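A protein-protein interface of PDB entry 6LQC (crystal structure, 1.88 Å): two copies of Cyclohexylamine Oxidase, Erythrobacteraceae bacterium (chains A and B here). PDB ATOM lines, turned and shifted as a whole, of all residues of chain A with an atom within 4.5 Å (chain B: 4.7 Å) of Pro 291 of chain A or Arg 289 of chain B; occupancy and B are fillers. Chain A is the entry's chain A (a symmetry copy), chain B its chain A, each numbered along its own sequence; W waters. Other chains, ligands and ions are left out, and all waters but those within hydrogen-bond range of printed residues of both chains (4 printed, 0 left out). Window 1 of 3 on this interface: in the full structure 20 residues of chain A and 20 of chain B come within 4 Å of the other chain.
The guanidinium group of Arg 289 of chain B lies within salt-bridge range of the side-chain carboxylate of Glu 181 of chain A, at 2.9 Å. The guanidinium group of Arg 294 of chain A lies close to the guanidinium group of Arg 289 of chain B (3.4 Å).
O of Pro 291 of chain A is in hydrogen-bond range of N of Phe 399 of chain A (3.0 Å). OE1 of Gln 285 of chain B sits at hydrogen-bond distance from NH1 of Arg 289 of chain B, at 2.9 Å. NH1 of Arg 294 of chain A is in salt-bridge range of OE1 of Glu 181 of chain A (2.9 Å).
Arg 289 of chain A touches Pro 291 of chain B (CG to CB, 3.8 Å). Pro 291 of chain A touches Arg 289 of chain B (CB to CG, 3.8 Å). Gln 285 of chain B touches Arg 294 of chain A.
Pro 291 of chain A touches one residue of chain B. Of chain A, only Glu 181 (2.9 Å), Pro 291 (3.8 Å) and Arg 294 (3.4 Å) come within 4 Å of Arg 289 of chain B. Printed residues of chain A within 4 Å of Pro 291 of chain B: Arg 289. Printed residues of chain B within 4 Å of Arg 289 of chain A: Pro 291 (3.8 Å). Of the printed residues of chain A, Gln 285 of chain B touches Arg 294. Of the printed residues of chain B, Glu 181 of chain A touches Arg 289 (2.9 Å). Of the printed residues of chain B, Arg 294 of chain A touches Gln 285 (3.5 Å) and Arg 289 (3.4 Å). Gly 293 of chain A touches none of the printed residues of chain B. The nearest residue of chain B that does not touch Pro 291 of chain A is Ala 288 of chain B (4.2 Å).
Of the 11 printed residues of chain B, 3 touch a printed residue of chain A. Printed residues of chain B that touch a printed residue of chain A: Gln 285, Arg 289 and Pro 291. Hydrophobic or aromatic side chains of chain B that line the printed part of chain A: Pro 291. Hydrophobic or aromatic side chains of chain A that line the printed part of chain B: Pro 291. Among the printed residues, 5 pairs touch across the chains.
Arg 289 of chain A touches Pro 291 of chain B, and with the chains exchanged Pro 291 of chain A touches Arg 289 of chain B.
Water W2 bridges the side-chain carboxylate of Glu 181 of chain A (2.6 Å) and the backbone carbonyl oxygen of Gly 403 of chain B (3.1 Å). Water W4 lies within hydrogen-bond range of the side-chain amide oxygen of Gln 285 of chain B (2.8 Å), the backbone carbonyl oxygen of Met 292 of chain A (2.9 Å) and the guanidinium group of Arg 294 of chain A (3.1 Å). Water W3 lies within hydrogen-bond range of NE2 of Gln 285 of chain B and O of Gly 293 of chain A. Water W1 lies within hydrogen-bond range of the guanidinium group (NH1) of Arg 289 of chain B (3.1 Å), the side-chain hydroxyl (OG) of Ser 407 of chain B (3.1 Å) and the guanidinium group (NH2) of Arg 294 of chain A (3.4 Å).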
ATOM      1  N   GLU A 181      -8.128  12.272  27.921  1.00  0.00           N
ATOM      2  CA  GLU A 181      -6.758  11.669  28.021  1.00  0.00           C
ATOM      3  C   GLU A 181      -6.529  11.005  29.384  1.00  0.00           C
ATOM      4  O   GLU A 181      -5.693  10.115  29.468  1.00  0.00           O
ATOM      5  CB  GLU A 181      -5.707  12.762  27.799  1.00  0.00           C
ATOM      6  CG  GLU A 181      -5.734  13.389  26.409  1.00  0.00           C
ATOM      7  CD  GLU A 181      -5.047  14.764  26.261  1.00  0.00           C
ATOM      8  OE1 GLU A 181      -4.658  15.362  27.270  1.00  0.00           O
ATOM      9  OE2 GLU A 181      -4.934  15.250  25.118  1.00  0.00           O
ATOM     10  N   ARG A 289       4.966   5.660  30.784  1.00  0.00           N
ATOM     11  CA  ARG A 289       3.552   5.853  30.353  1.00  0.00           C
ATOM     12  C   ARG A 289       2.807   6.841  31.257  1.00  0.00           C
ATOM     13  O   ARG A 289       1.587   7.095  30.961  1.00  0.00           O
ATOM     14  CB  ARG A 289       2.856   4.498  30.257  1.00  0.00           C
ATOM     15  CG  ARG A 289       3.365   3.649  29.102  1.00  0.00           C
ATOM     16  CD  ARG A 289       3.008   2.203  29.230  1.00  0.00           C
ATOM     17  NE  ARG A 289       1.601   1.933  29.526  1.00  0.00           N
ATOM     18  CZ  ARG A 289       1.163   0.837  30.117  1.00  0.00           C
ATOM     19  NH1 ARG A 289       1.991  -0.158  30.409  1.00  0.00           N
ATOM     20  NH2 ARG A 289      -0.123   0.729  30.391  1.00  0.00           N
ATOM     21  N   ALA A 290       3.410   7.338  32.336  1.00  0.00           N
ATOM     22  CA  ALA A 290       2.777   8.395  33.173  1.00  0.00           C
ATOM     23  C   ALA A 290       3.366   9.749  32.795  1.00  0.00           C
ATOM     24  O   ALA A 290       4.442  10.137  33.292  1.00  0.00           O
ATOM     25  CB  ALA A 290       2.955   8.115  34.620  1.00  0.00           C
ATOM     26  N   PRO A 291       2.760  10.503  31.852  1.00  0.00           N
ATOM     27  CA  PRO A 291       3.405  11.711  31.353  1.00  0.00           C
ATOM     28  C   PRO A 291       3.093  12.904  32.268  1.00  0.00           C
ATOM     29  O   PRO A 291       2.211  12.859  33.097  1.00  0.00           O
ATOM     30  CB  PRO A 291       2.761  11.970  29.985  1.00  0.00           C
ATOM     31  CG  PRO A 291       1.617  10.994  29.866  1.00  0.00           C
ATOM     32  CD  PRO A 291       1.450  10.302  31.207  1.00  0.00           C
ATOM     33  N   MET A 292       3.790  14.008  32.049  1.00  0.00           N
ATOM     34  CA  MET A 292       3.431  15.285  32.682  1.00  0.00           C
ATOM     35  C   MET A 292       2.197  15.792  31.926  1.00  0.00           C
ATOM     36  O   MET A 292       2.132  15.665  30.679  1.00  0.00           O
ATOM     37  CB  MET A 292       4.555  16.319  32.565  1.00  0.00           C
ATOM     38  CG  MET A 292       5.819  15.936  33.265  1.00  0.00           C
ATOM     39  SD  MET A 292       5.549  15.662  35.025  1.00  0.00           S
ATOM     40  CE  MET A 292       4.918  17.243  35.542  1.00  0.00           C
ATOM     41  N   GLY A 293       1.346  16.474  32.664  1.00  0.00           N
ATOM     42  CA  GLY A 293       0.306  17.346  32.121  1.00  0.00           C
ATOM     43  C   GLY A 293       0.978  18.535  31.428  1.00  0.00           C
ATOM     44  O   GLY A 293       2.251  18.656  31.439  1.00  0.00           O
ATOM     45  N   ARG A 294       0.171  19.397  30.850  1.00  0.00           N
ATOM     46  CA  ARG A 294       0.657  20.646  30.219  1.00  0.00           C
ATOM     47  C   ARG A 294      -0.117  21.802  30.834  1.00  0.00           C
ATOM     48  O   ARG A 294      -1.375  21.740  30.864  1.00  0.00           O
ATOM     49  CB  ARG A 294       0.561  20.524  28.697  1.00  0.00           C
ATOM     50  CG  ARG A 294      -0.811  20.147  28.145  1.00  0.00           C
ATOM     51  CD  ARG A 294      -0.658  19.407  26.828  1.00  0.00           C
ATOM     52  NE  ARG A 294      -1.918  19.075  26.159  1.00  0.00           N
ATOM     53  CZ  ARG A 294      -2.725  18.063  26.484  1.00  0.00           C
ATOM     54  NH1 ARG A 294      -2.387  17.184  27.413  1.00  0.00           N
ATOM     55  NH2 ARG A 294      -3.841  17.896  25.811  1.00  0.00           N
ATOM     56  N   VAL A 397       1.298  18.536  37.215  1.00  0.00           N
ATOM     57  CA  VAL A 397       1.464  17.185  37.785  1.00  0.00           C
ATOM     58  C   VAL A 397       1.666  16.146  36.679  1.00  0.00           C
ATOM     59  O   VAL A 397       1.318  16.373  35.511  1.00  0.00           O
ATOM     60  CB  VAL A 397       0.224  16.833  38.638  1.00  0.00           C
ATOM     61  CG1 VAL A 397       0.000  17.841  39.767  1.00  0.00           C
ATOM     62  CG2 VAL A 397      -1.027  16.736  37.777  1.00  0.00           C
ATOM     63  N   THR A 398       2.083  14.978  37.129  1.00  0.00           N
ATOM     64  CA  THR A 398       1.972  13.709  36.393  1.00  0.00           C
ATOM     65  C   THR A 398       0.479  13.339  36.292  1.00  0.00           C
ATOM     66  O   THR A 398      -0.219  13.464  37.280  1.00  0.00           O
ATOM     67  CB  THR A 398       2.760  12.618  37.120  1.00  0.00           C
ATOM     68  OG1 THR A 398       4.169  12.921  37.114  1.00  0.00           O
ATOM     69  CG2 THR A 398       2.575  11.263  36.481  1.00  0.00           C
ATOM     70  N   PHE A 399       0.060  12.832  35.143  1.00  0.00           N
ATOM     71  CA  PHE A 399      -1.249  12.149  34.996  1.00  0.00           C
ATOM     72  C   PHE A 399      -1.006  10.764  34.426  1.00  0.00           C
ATOM     73  O   PHE A 399       0.150  10.413  34.041  1.00  0.00           O
ATOM     74  CB  PHE A 399      -2.180  13.000  34.131  1.00  0.00           C
ATOM     75  CG  PHE A 399      -1.933  12.902  32.645  1.00  0.00           C
ATOM     76  CD1 PHE A 399      -1.059  13.783  32.018  1.00  0.00           C
ATOM     77  CD2 PHE A 399      -2.590  11.961  31.861  1.00  0.00           C
ATOM     78  CE1 PHE A 399      -0.873  13.728  30.642  1.00  0.00           C
ATOM     79  CE2 PHE A 399      -2.423  11.921  30.481  1.00  0.00           C
ATOM     80  CZ  PHE A 399      -1.546  12.788  29.874  1.00  0.00           C
ATOM     81  N   PRO A 401      -2.927   7.792  31.700  1.00  0.00           N
ATOM     82  CA  PRO A 401      -3.978   7.419  30.763  1.00  0.00           C
ATOM     83  C   PRO A 401      -4.567   6.070  31.177  1.00  0.00           C
ATOM     84  O   PRO A 401      -4.127   5.464  32.174  1.00  0.00           O
ATOM     85  CB  PRO A 401      -3.233   7.268  29.450  1.00  0.00           C
ATOM     86  CG  PRO A 401      -1.938   6.628  29.919  1.00  0.00           C
ATOM     87  CD  PRO A 401      -1.623   7.322  31.242  1.00  0.00           C
ATOM     88  N   GLN B 285       4.542  16.958  22.688  1.00  0.00           N
ATOM     89  CA  GLN B 285       3.472  16.087  23.256  1.00  0.00           C
ATOM     90  C   GLN B 285       3.541  14.686  22.657  1.00  0.00           C
ATOM     91  O   GLN B 285       3.509  13.678  23.419  1.00  0.00           O
ATOM     92  CB  GLN B 285       2.118  16.754  23.011  1.00  0.00           C
ATOM     93  CG  GLN B 285       1.935  18.008  23.872  1.00  0.00           C
ATOM     94  CD  GLN B 285       2.139  17.781  25.347  1.00  0.00           C
ATOM     95  OE1 GLN B 285       1.546  16.869  25.903  1.00  0.00           O
ATOM     96  NE2 GLN B 285       2.972  18.596  26.003  1.00  0.00           N
ATOM     97  N   LEU B 286       3.751  14.612  21.358  1.00  0.00           N
ATOM     98  CA  LEU B 286       3.860  13.325  20.635  1.00  0.00           C
ATOM     99  C   LEU B 286       4.995  12.503  21.216  1.00  0.00           C
ATOM    100  O   LEU B 286       4.798  11.299  21.515  1.00  0.00           O
ATOM    101  CB  LEU B 286       4.083  13.581  19.161  1.00  0.00           C
ATOM    102  CG  LEU B 286       4.175  12.305  18.349  1.00  0.00           C
ATOM    103  CD1 LEU B 286       2.819  11.605  18.361  1.00  0.00           C
ATOM    104  CD2 LEU B 286       4.580  12.647  16.932  1.00  0.00           C
ATOM    105  N   GLN B 287       6.183  13.105  21.375  1.00  0.00           N
ATOM    106  CA  GLN B 287       7.313  12.331  21.915  1.00  0.00           C
ATOM    107  C   GLN B 287       7.012  11.848  23.345  1.00  0.00           C
ATOM    108  O   GLN B 287       7.394  10.739  23.685  1.00  0.00           O
ATOM    109  CB  GLN B 287       8.612  13.153  21.830  1.00  0.00           C
ATOM    110  CG  GLN B 287       8.987  13.549  20.423  1.00  0.00           C
ATOM    111  CD  GLN B 287      10.376  14.151  20.292  1.00  0.00           C
ATOM    112  OE1 GLN B 287      11.009  13.994  19.261  1.00  0.00           O
ATOM    113  NE2 GLN B 287      10.871  14.766  21.341  1.00  0.00           N
ATOM    114  N   ALA B 288       6.408  12.669  24.181  1.00  0.00           N
ATOM    115  CA  ALA B 288       6.228  12.347  25.596  1.00  0.00           C
ATOM    116  C   ALA B 288       5.103  11.326  25.773  1.00  0.00           C
ATOM    117  O   ALA B 288       5.083  10.664  26.786  1.00  0.00           O
ATOM    118  CB  ALA B 288       5.943  13.613  26.352  1.00  0.00           C
ATOM    119  N   ARG B 289       4.150  11.257  24.865  1.00  0.00           N
ATOM    120  CA  ARG B 289       2.880  10.537  25.168  1.00  0.00           C
ATOM    121  C   ARG B 289       2.650   9.357  24.218  1.00  0.00           C
ATOM    122  O   ARG B 289       1.595   8.655  24.405  1.00  0.00           O
ATOM    123  CB  ARG B 289       1.719  11.526  25.175  1.00  0.00           C
ATOM    124  CG  ARG B 289       1.760  12.484  26.356  1.00  0.00           C
ATOM    125  CD  ARG B 289       0.897  13.690  26.170  1.00  0.00           C
ATOM    126  NE  ARG B 289      -0.474  13.413  25.741  1.00  0.00           N
ATOM    127  CZ  ARG B 289      -1.237  14.273  25.093  1.00  0.00           C
ATOM    128  NH1 ARG B 289      -0.823  15.513  24.860  1.00  0.00           N
ATOM    129  NH2 ARG B 289      -2.438  13.893  24.699  1.00  0.00           N
ATOM    130  N   ALA B 290       3.492   9.144  23.208  1.00  0.00           N
ATOM    131  CA  ALA B 290       3.385   7.942  22.335  1.00  0.00           C
ATOM    132  C   ALA B 290       4.405   6.904  22.790  1.00  0.00           C
ATOM    133  O   ALA B 290       5.588   6.960  22.401  1.00  0.00           O
ATOM    134  CB  ALA B 290       3.577   8.294  20.906  1.00  0.00           C
ATOM    135  N   PRO B 291       4.044   5.960  23.687  1.00  0.00           N
ATOM    136  CA  PRO B 291       5.049   5.075  24.265  1.00  0.00           C
ATOM    137  C   PRO B 291       5.296   3.870  23.347  1.00  0.00           C
ATOM    138  O   PRO B 291       4.543   3.594  22.439  1.00  0.00           O
ATOM    139  CB  PRO B 291       4.427   4.568  25.572  1.00  0.00           C
ATOM    140  CG  PRO B 291       2.994   5.038  25.568  1.00  0.00           C
ATOM    141  CD  PRO B 291       2.702   5.640  24.204  1.00  0.00           C
ATOM    142  N   PRO B 401      -2.234   6.319  23.266  1.00  0.00           N
ATOM    143  CA  PRO B 401      -3.429   6.251  24.095  1.00  0.00           C
ATOM    144  C   PRO B 401      -4.443   7.284  23.604  1.00  0.00           C
ATOM    145  O   PRO B 401      -4.175   8.029  22.641  1.00  0.00           O
ATOM    146  CB  PRO B 401      -2.920   6.648  25.469  1.00  0.00           C
ATOM    147  CG  PRO B 401      -1.926   7.738  25.109  1.00  0.00           C
ATOM    148  CD  PRO B 401      -1.251   7.238  23.833  1.00  0.00           C
ATOM    149  N   GLY B 403      -6.584  10.371  22.678  1.00  0.00           N
ATOM    150  CA  GLY B 403      -6.478  11.842  22.568  1.00  0.00           C
ATOM    151  C   GLY B 403      -5.205  12.286  21.867  1.00  0.00           C
ATOM    152  O   GLY B 403      -5.144  13.464  21.442  1.00  0.00           O
ATOM    153  N   LEU B 404      -4.224  11.403  21.638  1.00  0.00           N
ATOM    154  CA  LEU B 404      -2.922  11.879  21.054  1.00  0.00           C
ATOM    155  C   LEU B 404      -2.985  12.022  19.529  1.00  0.00           C
ATOM    156  O   LEU B 404      -2.525  13.073  19.020  1.00  0.00           O
ATOM    157  CB  LEU B 404      -1.787  10.933  21.444  1.00  0.00           C
ATOM    158  CG  LEU B 404      -0.375  11.470  21.188  1.00  0.00           C
ATOM    159  CD1 LEU B 404      -0.171  12.815  21.833  1.00  0.00           C
ATOM    160  CD2 LEU B 404       0.672  10.476  21.717  1.00  0.00           C
ATOM    161  N   SER B 407      -4.666  15.067  18.301  1.00  0.00           N
ATOM    162  CA  SER B 407      -4.195  16.374  18.798  1.00  0.00           C
ATOM    163  C   SER B 407      -2.728  16.648  18.380  1.00  0.00           C
ATOM    164  O   SER B 407      -2.332  17.804  18.363  1.00  0.00           O
ATOM    165  CB  SER B 407      -4.366  16.495  20.293  1.00  0.00           C
ATOM    166  OG  SER B 407      -3.519  15.596  20.980  1.00  0.00           O
HETATM  167  O   HOH W   1      -2.047  17.502  22.896  1.00  0.00           O
HETATM  168  O   HOH W   2      -6.624  15.555  23.156  1.00  0.00           O
HETATM  169  O   HOH W   3       3.661  18.257  28.852  1.00  0.00           O
HETATM  170  O   HOH W   4       0.427  16.659  28.501  1.00  0.00           O
